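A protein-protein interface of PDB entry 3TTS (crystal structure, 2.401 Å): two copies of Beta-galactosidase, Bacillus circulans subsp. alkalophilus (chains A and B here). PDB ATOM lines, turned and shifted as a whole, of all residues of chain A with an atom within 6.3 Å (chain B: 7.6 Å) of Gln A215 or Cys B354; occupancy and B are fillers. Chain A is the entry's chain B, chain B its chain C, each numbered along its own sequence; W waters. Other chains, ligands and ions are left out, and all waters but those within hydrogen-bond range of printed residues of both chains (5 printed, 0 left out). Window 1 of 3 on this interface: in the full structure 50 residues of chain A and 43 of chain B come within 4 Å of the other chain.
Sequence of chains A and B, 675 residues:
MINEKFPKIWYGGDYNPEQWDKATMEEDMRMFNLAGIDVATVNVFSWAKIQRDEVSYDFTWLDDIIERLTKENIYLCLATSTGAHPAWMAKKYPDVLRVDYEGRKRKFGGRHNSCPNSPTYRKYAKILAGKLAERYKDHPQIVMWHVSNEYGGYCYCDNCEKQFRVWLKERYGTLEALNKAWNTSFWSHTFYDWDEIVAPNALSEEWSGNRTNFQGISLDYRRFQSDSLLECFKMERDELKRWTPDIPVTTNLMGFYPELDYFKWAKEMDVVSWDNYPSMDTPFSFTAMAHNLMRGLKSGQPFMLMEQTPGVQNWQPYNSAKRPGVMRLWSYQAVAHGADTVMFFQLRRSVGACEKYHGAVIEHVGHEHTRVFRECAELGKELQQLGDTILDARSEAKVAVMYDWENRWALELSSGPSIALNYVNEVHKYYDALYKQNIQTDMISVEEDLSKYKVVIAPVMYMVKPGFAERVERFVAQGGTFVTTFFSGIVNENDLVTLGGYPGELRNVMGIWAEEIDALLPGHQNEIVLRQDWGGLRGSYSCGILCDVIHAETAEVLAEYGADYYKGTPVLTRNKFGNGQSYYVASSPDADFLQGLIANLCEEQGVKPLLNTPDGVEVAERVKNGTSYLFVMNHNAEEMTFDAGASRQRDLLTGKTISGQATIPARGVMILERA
The backbone NH (N) of Cys B354 lies close to the backbone carbonyl oxygen (O) of Asn A213 (3.1 Å).
O of Ala B353 sits close to OE1 of Gln A215.
N of Cys B354 is in hydrogen-bond range of OE1 of Gln A215 (2.8 Å).
The backbone carbonyl oxygen (O) of Cys B354 lies within hydrogen-bond range of the side-chain hydroxyl (OG) of Ser A415.
N of Gly A416 lies within hydrogen-bond range of O of Asn B314.
The side-chain hydroxyl of Tyr A462 lies within hydrogen-bond range of the side-chain amino group of Lys B356 (2.7 Å).
The side-chain hydroxyl (OH) of Tyr A462 sits at hydrogen-bond distance from the side-chain hydroxyl (OH) of Tyr B357.
The side-chain carboxylate (OD2) of Asp A495 is in salt-bridge range of the side-chain amino group (NZ) of Lys B356, at 3.0 Å.
OE2 of Glu A205 lies within hydrogen-bond range of ND2 of Asn A213 (2.9 Å).
The backbone carbonyl oxygen (O) of Asn A213 sits close to the side-chain amide oxygen (OE1) of Gln A215 (3.5 Å).
The backbone carbonyl oxygen of Phe A214 is in hydrogen-bond range of the side-chain hydroxyl of Ser A218 (3.4 Å).
OG of Ser A414 is in hydrogen-bond range of O of Gly A416 (2.5 Å).
The backbone carbonyl oxygen of Cys B354 is in hydrogen-bond range of the side-chain amide nitrogen of Asn B314, at 2.8 Å.
The side-chain amino group (NZ) of Lys B356 lies close to the side-chain hydroxyl (OH) of Tyr B357, at 3.3 Å.
Arg B111 touches Trp A187.
CZ2 of Trp A187 touches OE1 of Glu B355, at 3.6 Å.
Trp B315 touches Trp A207 (CH2 to CZ2, 3.4 Å).
O of Thr A212 touches CH2 of Trp B315, 3.8 Å away.
Cys B354 touches Thr A212 (CB to O, 3.5 Å).
CB of Ala B353 touches O of Asn A213, at 3.4 Å.
Phe A214 touches Ala B353.
Ser A414 touches Tyr B357.
Ser A415 touches Asn B314 (C to O, 3.4 Å).
Ser A415 touches Trp B315 (OG to CH2, 3.6 Å).
Printed residues of chain B within 4 Å of Phe A186: Ala B353 and Glu B355.
Printed residues of chain B within 4 Å of Trp A187: Arg B111 (3.2 Å), Cys B354 (3.5 Å) and Glu B355 (3.6 Å).
Printed residues of chain B within 4 Å of Thr A212: Trp B315 (3.8 Å) and Cys B354 (3.5 Å).
Gln A215 touches two residues of chain B.
Leu A413 touches none of the printed residues of chain B.
Of the printed residues of chain B, Ser A414 touches Tyr B357.
Of chain A, only Trp A187 (3.5 Å), Thr A212 (3.5 Å), Asn A213 (3.1 Å), Gln A215 (2.8 Å) and Ser A415 (3.4 Å) come within 4 Å of Cys B354.
The nearest residue of chain A that does not touch Cys B354 is Phe A186 (4.2 Å).
The nearest printed residue of chain A that does not touch Asn B314 is Ser A414 (6.4 Å).
Printed residues of chain B that touch a printed residue of chain A: Arg B111, Asn B314, Trp B315, Ala B353, Cys B354, Glu B355, Lys B356 and Tyr B357.
Hydrophobic or aromatic side chains of chain B that line the printed part of chain A: Trp B315, Ala B353 and Tyr B357.
Among the printed residues, 21 pairs touch across the chains.
Among the printed residues, Asp or Glu carboxylates within 4 Å of a Lys or Arg side-chain nitrogen of the other chain: Asp A495 with Lys B356 (3.0 Å).
No position is printed for both chains.
Of the 21 pairs that touch across the chains among the printed residues, none has its exchanged pair printed and touching as well.
Water W3 lies within hydrogen-bond range of O of Ser A415, O of Cys B354, N of Tyr B357 and N of Lys B356.
Water W2 bridges OE2 of Glu B355 (2.6 Å) and NE1 of Trp A187 (3.0 Å).
Water W5 lies within hydrogen-bond range of the side-chain carboxylate (OD2) of Asp A495 (2.7 Å), the backbone carbonyl oxygen (O) of Ala A410 (2.8 Å), the side-chain amino group (NZ) of Lys B356 (2.9 Å) and the side-chain hydroxyl (OH) of Tyr A462 (3.2 Å).
Water W4 bridges OD2 of Asp A495 (2.7 Å) and O of Gly B352 (2.9 Å).
Water W1 lies within hydrogen-bond range of N of Ser A415 (2.9 Å), OG of Ser A414 (3.2 Å) and NZ of Lys B356 (3.3 Å).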
ATOM      1  N   PHE A 186      19.562 -30.537 -35.638  1.00  0.00           N
ATOM      2  CA  PHE A 186      18.729 -31.275 -34.700  1.00  0.00           C
ATOM      3  C   PHE A 186      17.389 -31.689 -35.342  1.00  0.00           C
ATOM      4  O   PHE A 186      16.760 -30.915 -36.063  1.00  0.00           O
ATOM      5  CB  PHE A 186      18.492 -30.378 -33.487  1.00  0.00           C
ATOM      6  CG  PHE A 186      17.694 -31.009 -32.388  1.00  0.00           C
ATOM      7  CD1 PHE A 186      18.271 -31.970 -31.555  1.00  0.00           C
ATOM      8  CD2 PHE A 186      16.389 -30.595 -32.140  1.00  0.00           C
ATOM      9  CE1 PHE A 186      17.546 -32.545 -30.523  1.00  0.00           C
ATOM     10  CE2 PHE A 186      15.653 -31.162 -31.098  1.00  0.00           C
ATOM     11  CZ  PHE A 186      16.239 -32.135 -30.284  1.00  0.00           C
ATOM     12  N   TRP A 187      16.965 -32.921 -35.073  1.00  0.00           N
ATOM     13  CA  TRP A 187      15.720 -33.459 -35.609  1.00  0.00           C
ATOM     14  C   TRP A 187      15.553 -33.183 -37.109  1.00  0.00           C
ATOM     15  O   TRP A 187      14.453 -32.881 -37.579  1.00  0.00           O
ATOM     16  CB  TRP A 187      14.505 -32.960 -34.800  1.00  0.00           C
ATOM     17  CG  TRP A 187      14.472 -33.475 -33.365  1.00  0.00           C
ATOM     18  CD1 TRP A 187      15.407 -34.273 -32.748  1.00  0.00           C
ATOM     19  CD2 TRP A 187      13.455 -33.225 -32.380  1.00  0.00           C
ATOM     20  NE1 TRP A 187      15.027 -34.534 -31.454  1.00  0.00           N
ATOM     21  CE2 TRP A 187      13.839 -33.898 -31.201  1.00  0.00           C
ATOM     22  CE3 TRP A 187      12.259 -32.493 -32.382  1.00  0.00           C
ATOM     23  CZ2 TRP A 187      13.077 -33.858 -30.032  1.00  0.00           C
ATOM     24  CZ3 TRP A 187      11.496 -32.460 -31.226  1.00  0.00           C
ATOM     25  CH2 TRP A 187      11.909 -33.142 -30.064  1.00  0.00           C
ATOM     26  N   GLU A 205       5.177 -26.655 -34.182  1.00  0.00           N
ATOM     27  CA  GLU A 205       6.302 -26.796 -33.290  1.00  0.00           C
ATOM     28  C   GLU A 205       5.898 -26.673 -31.826  1.00  0.00           C
ATOM     29  O   GLU A 205       6.641 -27.095 -30.943  1.00  0.00           O
ATOM     30  CB  GLU A 205       7.346 -25.739 -33.659  1.00  0.00           C
ATOM     31  CG  GLU A 205       8.765 -26.210 -33.639  1.00  0.00           C
ATOM     32  CD  GLU A 205       9.022 -27.435 -34.512  1.00  0.00           C
ATOM     33  OE1 GLU A 205       9.390 -27.290 -35.708  1.00  0.00           O
ATOM     34  OE2 GLU A 205       8.886 -28.548 -33.967  1.00  0.00           O
ATOM     35  N   TRP A 207       2.918 -26.444 -28.365  1.00  0.00           N
ATOM     36  CA  TRP A 207       1.680 -26.948 -27.786  1.00  0.00           C
ATOM     37  C   TRP A 207       1.448 -26.330 -26.420  1.00  0.00           C
ATOM     38  O   TRP A 207       2.374 -25.798 -25.806  1.00  0.00           O
ATOM     39  CB  TRP A 207       1.666 -28.480 -27.715  1.00  0.00           C
ATOM     40  CG  TRP A 207       2.739 -29.054 -26.851  1.00  0.00           C
ATOM     41  CD1 TRP A 207       2.634 -29.394 -25.538  1.00  0.00           C
ATOM     42  CD2 TRP A 207       4.087 -29.356 -27.236  1.00  0.00           C
ATOM     43  NE1 TRP A 207       3.826 -29.877 -25.076  1.00  0.00           N
ATOM     44  CE2 TRP A 207       4.736 -29.876 -26.101  1.00  0.00           C
ATOM     45  CE3 TRP A 207       4.804 -29.236 -28.426  1.00  0.00           C
ATOM     46  CZ2 TRP A 207       6.070 -30.279 -26.120  1.00  0.00           C
ATOM     47  CZ3 TRP A 207       6.139 -29.630 -28.442  1.00  0.00           C
ATOM     48  CH2 TRP A 207       6.755 -30.143 -27.300  1.00  0.00           C
ATOM     49  N   THR A 212       7.586 -25.950 -26.752  1.00  0.00           N
ATOM     50  CA  THR A 212       8.074 -25.926 -28.126  1.00  0.00           C
ATOM     51  C   THR A 212       9.188 -26.948 -28.349  1.00  0.00           C
ATOM     52  O   THR A 212       9.991 -27.204 -27.460  1.00  0.00           O
ATOM     53  CB  THR A 212       8.541 -24.487 -28.524  1.00  0.00           C
ATOM     54  OG1 THR A 212       8.990 -24.456 -29.886  1.00  0.00           O
ATOM     55  CG2 THR A 212       9.660 -23.993 -27.601  1.00  0.00           C
ATOM     56  N   ASN A 213       9.234 -27.531 -29.542  1.00  0.00           N
ATOM     57  CA  ASN A 213      10.363 -28.369 -29.949  1.00  0.00           C
ATOM     58  C   ASN A 213      11.617 -27.572 -30.318  1.00  0.00           C
ATOM     59  O   ASN A 213      12.742 -28.060 -30.200  1.00  0.00           O
ATOM     60  CB  ASN A 213       9.977 -29.189 -31.170  1.00  0.00           C
ATOM     61  CG  ASN A 213       8.836 -30.116 -30.893  1.00  0.00           C
ATOM     62  OD1 ASN A 213       8.828 -30.797 -29.874  1.00  0.00           O
ATOM     63  ND2 ASN A 213       7.845 -30.138 -31.787  1.00  0.00           N
ATOM     64  N   PHE A 214      11.405 -26.353 -30.804  1.00  0.00           N
ATOM     65  CA  PHE A 214      12.479 -25.570 -31.400  1.00  0.00           C
ATOM     66  C   PHE A 214      12.400 -24.134 -30.928  1.00  0.00           C
ATOM     67  O   PHE A 214      11.780 -23.291 -31.584  1.00  0.00           O
ATOM     68  CB  PHE A 214      12.389 -25.634 -32.933  1.00  0.00           C
ATOM     69  CG  PHE A 214      13.384 -26.575 -33.557  1.00  0.00           C
ATOM     70  CD1 PHE A 214      13.091 -27.927 -33.696  1.00  0.00           C
ATOM     71  CD2 PHE A 214      14.619 -26.106 -33.995  1.00  0.00           C
ATOM     72  CE1 PHE A 214      14.011 -28.801 -34.259  1.00  0.00           C
ATOM     73  CE2 PHE A 214      15.552 -26.977 -34.571  1.00  0.00           C
ATOM     74  CZ  PHE A 214      15.252 -28.324 -34.699  1.00  0.00           C
ATOM     75  N   GLN A 215      13.016 -23.841 -29.796  1.00  0.00           N
ATOM     76  CA  GLN A 215      12.804 -22.515 -29.218  1.00  0.00           C
ATOM     77  C   GLN A 215      13.396 -21.354 -30.031  1.00  0.00           C
ATOM     78  O   GLN A 215      12.886 -20.244 -29.966  1.00  0.00           O
ATOM     79  CB  GLN A 215      13.151 -22.431 -27.719  1.00  0.00           C
ATOM     80  CG  GLN A 215      14.095 -23.449 -27.190  1.00  0.00           C
ATOM     81  CD  GLN A 215      13.488 -24.824 -27.034  1.00  0.00           C
ATOM     82  OE1 GLN A 215      13.769 -25.708 -27.834  1.00  0.00           O
ATOM     83  NE2 GLN A 215      12.683 -25.026 -25.983  1.00  0.00           N
ATOM     84  N   GLY A 216      14.441 -21.620 -30.816  1.00  0.00           N
ATOM     85  CA  GLY A 216      14.960 -20.632 -31.742  1.00  0.00           C
ATOM     86  C   GLY A 216      13.906 -20.097 -32.718  1.00  0.00           C
ATOM     87  O   GLY A 216      13.847 -18.901 -32.978  1.00  0.00           O
ATOM     88  N   ILE A 217      13.081 -20.984 -33.272  1.00  0.00           N
ATOM     89  CA  ILE A 217      11.985 -20.564 -34.148  1.00  0.00           C
ATOM     90  C   ILE A 217      10.911 -19.808 -33.361  1.00  0.00           C
ATOM     91  O   ILE A 217      10.497 -18.715 -33.756  1.00  0.00           O
ATOM     92  CB  ILE A 217      11.364 -21.770 -34.906  1.00  0.00           C
ATOM     93  CG1 ILE A 217      12.479 -22.608 -35.558  1.00  0.00           C
ATOM     94  CG2 ILE A 217      10.348 -21.301 -35.933  1.00  0.00           C
ATOM     95  CD1 ILE A 217      12.000 -23.841 -36.307  1.00  0.00           C
ATOM     96  N   SER A 218      10.478 -20.373 -32.235  1.00  0.00           N
ATOM     97  CA  SER A 218       9.457 -19.728 -31.405  1.00  0.00           C
ATOM     98  C   SER A 218       9.897 -18.355 -30.892  1.00  0.00           C
ATOM     99  O   SER A 218       9.093 -17.425 -30.818  1.00  0.00           O
ATOM    100  CB  SER A 218       9.089 -20.620 -30.225  1.00  0.00           C
ATOM    101  OG  SER A 218       8.793 -21.924 -30.686  1.00  0.00           O
ATOM    102  N   LEU A 219      11.173 -18.237 -30.538  1.00  0.00           N
ATOM    103  CA  LEU A 219      11.720 -16.967 -30.086  1.00  0.00           C
ATOM    104  C   LEU A 219      11.634 -15.940 -31.215  1.00  0.00           C
ATOM    105  O   LEU A 219      11.102 -14.840 -31.030  1.00  0.00           O
ATOM    106  CB  LEU A 219      13.172 -17.144 -29.616  1.00  0.00           C
ATOM    107  CG  LEU A 219      13.908 -15.878 -29.176  1.00  0.00           C
ATOM    108  CD1 LEU A 219      13.273 -15.300 -27.908  1.00  0.00           C
ATOM    109  CD2 LEU A 219      15.408 -16.151 -28.963  1.00  0.00           C
ATOM    110  N   ASP A 220      12.128 -16.321 -32.393  1.00  0.00           N
ATOM    111  CA  ASP A 220      12.085 -15.446 -33.561  1.00  0.00           C
ATOM    112  C   ASP A 220      10.680 -15.066 -33.997  1.00  0.00           C
ATOM    113  O   ASP A 220      10.459 -13.929 -34.421  1.00  0.00           O
ATOM    114  CB  ASP A 220      12.854 -16.046 -34.731  1.00  0.00           C
ATOM    115  CG  ASP A 220      14.323 -15.680 -34.702  1.00  0.00           C
ATOM    116  OD1 ASP A 220      15.060 -16.139 -35.595  1.00  0.00           O
ATOM    117  OD2 ASP A 220      14.741 -14.930 -33.784  1.00  0.00           O
ATOM    118  N   ALA A 410      12.698 -16.551 -24.077  1.00  0.00           N
ATOM    119  CA  ALA A 410      13.581 -17.703 -24.102  1.00  0.00           C
ATOM    120  C   ALA A 410      13.388 -18.579 -22.860  1.00  0.00           C
ATOM    121  O   ALA A 410      13.380 -19.802 -22.954  1.00  0.00           O
ATOM    122  CB  ALA A 410      15.020 -17.275 -24.238  1.00  0.00           C
ATOM    123  N   LEU A 413       9.966 -20.587 -22.847  1.00  0.00           N
ATOM    124  CA  LEU A 413       9.856 -21.584 -23.903  1.00  0.00           C
ATOM    125  C   LEU A 413      10.791 -22.757 -23.629  1.00  0.00           C
ATOM    126  O   LEU A 413      10.626 -23.854 -24.181  1.00  0.00           O
ATOM    127  CB  LEU A 413      10.191 -20.967 -25.261  1.00  0.00           C
ATOM    128  CG  LEU A 413       9.176 -19.968 -25.831  1.00  0.00           C
ATOM    129  CD1 LEU A 413       9.826 -19.120 -26.941  1.00  0.00           C
ATOM    130  CD2 LEU A 413       7.904 -20.669 -26.335  1.00  0.00           C
ATOM    131  N   SER A 414      11.778 -22.518 -22.770  1.00  0.00           N
ATOM    132  CA  SER A 414      12.772 -23.531 -22.485  1.00  0.00           C
ATOM    133  C   SER A 414      12.179 -24.793 -21.861  1.00  0.00           C
ATOM    134  O   SER A 414      11.225 -24.730 -21.078  1.00  0.00           O
ATOM    135  CB  SER A 414      13.860 -22.967 -21.576  1.00  0.00           C
ATOM    136  OG  SER A 414      14.682 -24.010 -21.086  1.00  0.00           O
ATOM    137  N   SER A 415      12.761 -25.939 -22.195  1.00  0.00           N
ATOM    138  CA  SER A 415      12.437 -27.171 -21.474  1.00  0.00           C
ATOM    139  C   SER A 415      13.668 -27.907 -20.924  1.00  0.00           C
ATOM    140  O   SER A 415      14.546 -28.300 -21.690  1.00  0.00           O
ATOM    141  CB  SER A 415      11.646 -28.100 -22.391  1.00  0.00           C
ATOM    142  OG  SER A 415      12.161 -28.055 -23.703  1.00  0.00           O
ATOM    143  N   GLY A 416      13.792 -28.048 -19.608  1.00  0.00           N
ATOM    144  CA  GLY A 416      13.119 -27.244 -18.614  1.00  0.00           C
ATOM    145  C   GLY A 416      14.092 -26.129 -18.227  1.00  0.00           C
ATOM    146  O   GLY A 416      14.207 -25.153 -18.964  1.00  0.00           O
ATOM    147  N   TYR A 462      19.416 -15.229 -18.116  1.00  0.00           N
ATOM    148  CA  TYR A 462      19.622 -16.441 -18.903  1.00  0.00           C
ATOM    149  C   TYR A 462      20.241 -16.131 -20.264  1.00  0.00           C
ATOM    150  O   TYR A 462      21.223 -16.768 -20.673  1.00  0.00           O
ATOM    151  CB  TYR A 462      18.265 -17.164 -19.036  1.00  0.00           C
ATOM    152  CG  TYR A 462      18.163 -18.297 -20.049  1.00  0.00           C
ATOM    153  CD1 TYR A 462      18.667 -19.569 -19.767  1.00  0.00           C
ATOM    154  CD2 TYR A 462      17.503 -18.101 -21.267  1.00  0.00           C
ATOM    155  CE1 TYR A 462      18.553 -20.619 -20.698  1.00  0.00           C
ATOM    156  CE2 TYR A 462      17.377 -19.133 -22.194  1.00  0.00           C
ATOM    157  CZ  TYR A 462      17.908 -20.388 -21.907  1.00  0.00           C
ATOM    158  OH  TYR A 462      17.783 -21.388 -22.836  1.00  0.00           O
ATOM    159  N   ASN A 494      20.265 -15.911 -29.911  1.00  0.00           N
ATOM    160  CA  ASN A 494      19.517 -16.943 -30.631  1.00  0.00           C
ATOM    161  C   ASN A 494      19.082 -18.121 -29.775  1.00  0.00           C
ATOM    162  O   ASN A 494      18.611 -19.124 -30.300  1.00  0.00           O
ATOM    163  CB  ASN A 494      20.319 -17.452 -31.827  1.00  0.00           C
ATOM    164  CG  ASN A 494      20.297 -16.488 -32.989  1.00  0.00           C
ATOM    165  OD1 ASN A 494      19.225 -16.135 -33.489  1.00  0.00           O
ATOM    166  ND2 ASN A 494      21.470 -16.035 -33.409  1.00  0.00           N
ATOM    167  N   ASP A 495      19.252 -18.001 -28.463  1.00  0.00           N
ATOM    168  CA  ASP A 495      18.975 -19.104 -27.532  1.00  0.00           C
ATOM    169  C   ASP A 495      19.904 -20.301 -27.757  1.00  0.00           C
ATOM    170  O   ASP A 495      19.545 -21.433 -27.421  1.00  0.00           O
ATOM    171  CB  ASP A 495      17.500 -19.554 -27.587  1.00  0.00           C
ATOM    172  CG  ASP A 495      17.072 -20.335 -26.326  1.00  0.00           C
ATOM    173  OD1 ASP A 495      17.409 -19.887 -25.217  1.00  0.00           O
ATOM    174  OD2 ASP A 495      16.407 -21.397 -26.432  1.00  0.00           O
ATOM    175  N   ARG B 111       8.871 -34.284 -34.660  1.00  0.00           N
ATOM    176  CA  ARG B 111       9.465 -35.521 -35.143  1.00  0.00           C
ATOM    177  C   ARG B 111       8.515 -36.671 -34.849  1.00  0.00           C
ATOM    178  O   ARG B 111       7.494 -36.482 -34.190  1.00  0.00           O
ATOM    179  CB  ARG B 111      10.776 -35.780 -34.410  1.00  0.00           C
ATOM    180  CG  ARG B 111      10.555 -35.931 -32.916  1.00  0.00           C
ATOM    181  CD  ARG B 111      11.769 -36.510 -32.228  1.00  0.00           C
ATOM    182  NE  ARG B 111      11.540 -36.614 -30.793  1.00  0.00           N
ATOM    183  CZ  ARG B 111      12.423 -37.120 -29.939  1.00  0.00           C
ATOM    184  NH1 ARG B 111      13.588 -37.574 -30.383  1.00  0.00           N
ATOM    185  NH2 ARG B 111      12.138 -37.181 -28.648  1.00  0.00           N
ATOM    186  N   ASN B 314      14.845 -33.523 -19.602  1.00  0.00           N
ATOM    187  CA  ASN B 314      14.427 -32.181 -20.001  1.00  0.00           C
ATOM    188  C   ASN B 314      12.920 -31.986 -19.960  1.00  0.00           C
ATOM    189  O   ASN B 314      12.445 -30.867 -19.793  1.00  0.00           O
ATOM    190  CB  ASN B 314      14.975 -31.818 -21.390  1.00  0.00           C
ATOM    191  CG  ASN B 314      14.403 -32.686 -22.486  1.00  0.00           C
ATOM    192  OD1 ASN B 314      14.226 -33.902 -22.313  1.00  0.00           O
ATOM    193  ND2 ASN B 314      14.093 -32.065 -23.627  1.00  0.00           N
ATOM    194  N   TRP B 315      12.166 -33.071 -20.095  1.00  0.00           N
ATOM    195  CA  TRP B 315      10.706 -32.958 -20.213  1.00  0.00           C
ATOM    196  C   TRP B 315       9.877 -33.221 -18.951  1.00  0.00           C
ATOM    197  O   TRP B 315       8.661 -33.031 -18.965  1.00  0.00           O
ATOM    198  CB  TRP B 315      10.184 -33.800 -21.379  1.00  0.00           C
ATOM    199  CG  TRP B 315      10.428 -33.164 -22.733  1.00  0.00           C
ATOM    200  CD1 TRP B 315      11.234 -33.641 -23.732  1.00  0.00           C
ATOM    201  CD2 TRP B 315       9.860 -31.938 -23.228  1.00  0.00           C
ATOM    202  NE1 TRP B 315      11.198 -32.796 -24.815  1.00  0.00           N
ATOM    203  CE2 TRP B 315      10.367 -31.741 -24.536  1.00  0.00           C
ATOM    204  CE3 TRP B 315       8.975 -30.989 -22.694  1.00  0.00           C
ATOM    205  CZ2 TRP B 315      10.022 -30.630 -25.319  1.00  0.00           C
ATOM    206  CZ3 TRP B 315       8.632 -29.882 -23.465  1.00  0.00           C
ATOM    207  CH2 TRP B 315       9.156 -29.714 -24.770  1.00  0.00           C
ATOM    208  N   SER B 350      23.468 -31.249 -26.918  1.00  0.00           N
ATOM    209  CA  SER B 350      23.187 -30.334 -28.012  1.00  0.00           C
ATOM    210  C   SER B 350      23.084 -28.903 -27.467  1.00  0.00           C
ATOM    211  O   SER B 350      23.101 -28.675 -26.246  1.00  0.00           O
ATOM    212  CB  SER B 350      21.919 -30.743 -28.762  1.00  0.00           C
ATOM    213  OG  SER B 350      20.809 -30.759 -27.871  1.00  0.00           O
ATOM    214  N   VAL B 351      22.923 -27.948 -28.373  1.00  0.00           N
ATOM    215  CA  VAL B 351      23.322 -26.584 -28.080  1.00  0.00           C
ATOM    216  C   VAL B 351      22.284 -25.442 -28.110  1.00  0.00           C
ATOM    217  O   VAL B 351      22.513 -24.425 -27.477  1.00  0.00           O
ATOM    218  CB  VAL B 351      24.571 -26.207 -28.941  1.00  0.00           C
ATOM    219  CG1 VAL B 351      24.203 -25.273 -30.098  1.00  0.00           C
ATOM    220  CG2 VAL B 351      25.631 -25.605 -28.080  1.00  0.00           C
ATOM    221  N   GLY B 352      21.144 -25.554 -28.780  1.00  0.00           N
ATOM    222  CA  GLY B 352      20.566 -26.741 -29.376  1.00  0.00           C
ATOM    223  C   GLY B 352      19.133 -26.246 -29.467  1.00  0.00           C
ATOM    224  O   GLY B 352      18.900 -25.056 -29.302  1.00  0.00           O
ATOM    225  N   ALA B 353      18.165 -27.108 -29.709  1.00  0.00           N
ATOM    226  CA  ALA B 353      16.769 -26.673 -29.588  1.00  0.00           C
ATOM    227  C   ALA B 353      16.203 -27.187 -28.247  1.00  0.00           C
ATOM    228  O   ALA B 353      16.727 -26.829 -27.195  1.00  0.00           O
ATOM    229  CB  ALA B 353      15.936 -27.153 -30.791  1.00  0.00           C
ATOM    230  N   CYS B 354      15.180 -28.047 -28.261  1.00  0.00           N
ATOM    231  CA  CYS B 354      14.505 -28.389 -26.992  1.00  0.00           C
ATOM    232  C   CYS B 354      15.222 -29.420 -26.135  1.00  0.00           C
ATOM    233  O   CYS B 354      14.768 -29.742 -25.040  1.00  0.00           O
ATOM    234  CB  CYS B 354      13.057 -28.840 -27.212  1.00  0.00           C
ATOM    235  SG  CYS B 354      12.921 -30.471 -27.982  1.00  0.00           S
ATOM    236  N   GLU B 355      16.341 -29.942 -26.617  1.00  0.00           N
ATOM    237  CA  GLU B 355      17.080 -30.913 -25.826  1.00  0.00           C
ATOM    238  C   GLU B 355      18.416 -30.420 -25.250  1.00  0.00           C
ATOM    239  O   GLU B 355      19.173 -31.210 -24.688  1.00  0.00           O
ATOM    240  CB  GLU B 355      17.234 -32.226 -26.591  1.00  0.00           C
ATOM    241  CG  GLU B 355      15.940 -33.017 -26.640  1.00  0.00           C
ATOM    242  CD  GLU B 355      16.041 -34.270 -27.487  1.00  0.00           C
ATOM    243  OE1 GLU B 355      15.140 -35.131 -27.386  1.00  0.00           O
ATOM    244  OE2 GLU B 355      17.018 -34.395 -28.257  1.00  0.00           O
ATOM    245  N   LYS B 356      18.686 -29.120 -25.350  1.00  0.00           N
ATOM    246  CA  LYS B 356      19.948 -28.571 -24.846  1.00  0.00           C
ATOM    247  C   LYS B 356      20.149 -28.760 -23.333  1.00  0.00           C
ATOM    248  O   LYS B 356      21.288 -28.860 -22.867  1.00  0.00           O
ATOM    249  CB  LYS B 356      20.113 -27.091 -25.239  1.00  0.00           C
ATOM    250  CG  LYS B 356      18.995 -26.158 -24.789  1.00  0.00           C
ATOM    251  CD  LYS B 356      19.149 -24.789 -25.449  1.00  0.00           C
ATOM    252  CE  LYS B 356      17.810 -24.116 -25.715  1.00  0.00           C
ATOM    253  NZ  LYS B 356      17.347 -23.439 -24.497  1.00  0.00           N
ATOM    254  N   TYR B 357      19.061 -28.818 -22.567  1.00  0.00           N
ATOM    255  CA  TYR B 357      19.187 -29.083 -21.135  1.00  0.00           C
ATOM    256  C   TYR B 357      18.854 -30.519 -20.779  1.00  0.00           C
ATOM    257  O   TYR B 357      18.539 -30.829 -19.632  1.00  0.00           O
ATOM    258  CB  TYR B 357      18.419 -28.059 -20.294  1.00  0.00           C
ATOM    259  CG  TYR B 357      18.775 -26.681 -20.750  1.00  0.00           C
ATOM    260  CD1 TYR B 357      20.110 -26.298 -20.869  1.00  0.00           C
ATOM    261  CD2 TYR B 357      17.789 -25.792 -21.156  1.00  0.00           C
ATOM    262  CE1 TYR B 357      20.443 -25.047 -21.334  1.00  0.00           C
ATOM    263  CE2 TYR B 357      18.104 -24.546 -21.623  1.00  0.00           C
ATOM    264  CZ  TYR B 357      19.427 -24.173 -21.718  1.00  0.00           C
ATOM    265  OH  TYR B 357      19.717 -22.922 -22.202  1.00  0.00           O
ATOM    266  N   HIS B 358      18.945 -31.397 -21.776  1.00  0.00           N
ATOM    267  CA  HIS B 358      18.976 -32.829 -21.507  1.00  0.00           C
ATOM    268  C   HIS B 358      20.423 -33.262 -21.217  1.00  0.00           C
ATOM    269  O   HIS B 358      21.354 -32.846 -21.905  1.00  0.00           O
ATOM    270  CB  HIS B 358      18.410 -33.619 -22.688  1.00  0.00           C
ATOM    271  CG  HIS B 358      18.297 -35.089 -22.430  1.00  0.00           C
ATOM    272  ND1 HIS B 358      17.084 -35.746 -22.374  1.00  0.00           N
ATOM    273  CD2 HIS B 358      19.245 -36.029 -22.195  1.00  0.00           C
ATOM    274  CE1 HIS B 358      17.291 -37.027 -22.123  1.00  0.00           C
ATOM    275  NE2 HIS B 358      18.592 -37.224 -22.013  1.00  0.00           N
HETATM  276  O   HOH W   1      15.309 -25.872 -23.638  1.00  0.00           O
HETATM  277  O   HOH W   2      16.948 -36.293 -29.966  1.00  0.00           O
HETATM  278  O   HOH W   3      16.320 -28.287 -23.370  1.00  0.00           O
HETATM  279  O   HOH W   4      17.290 -22.749 -28.637  1.00  0.00           O
HETATM  280  O   HOH W   5      14.944 -21.829 -24.170  1.00  0.00           O
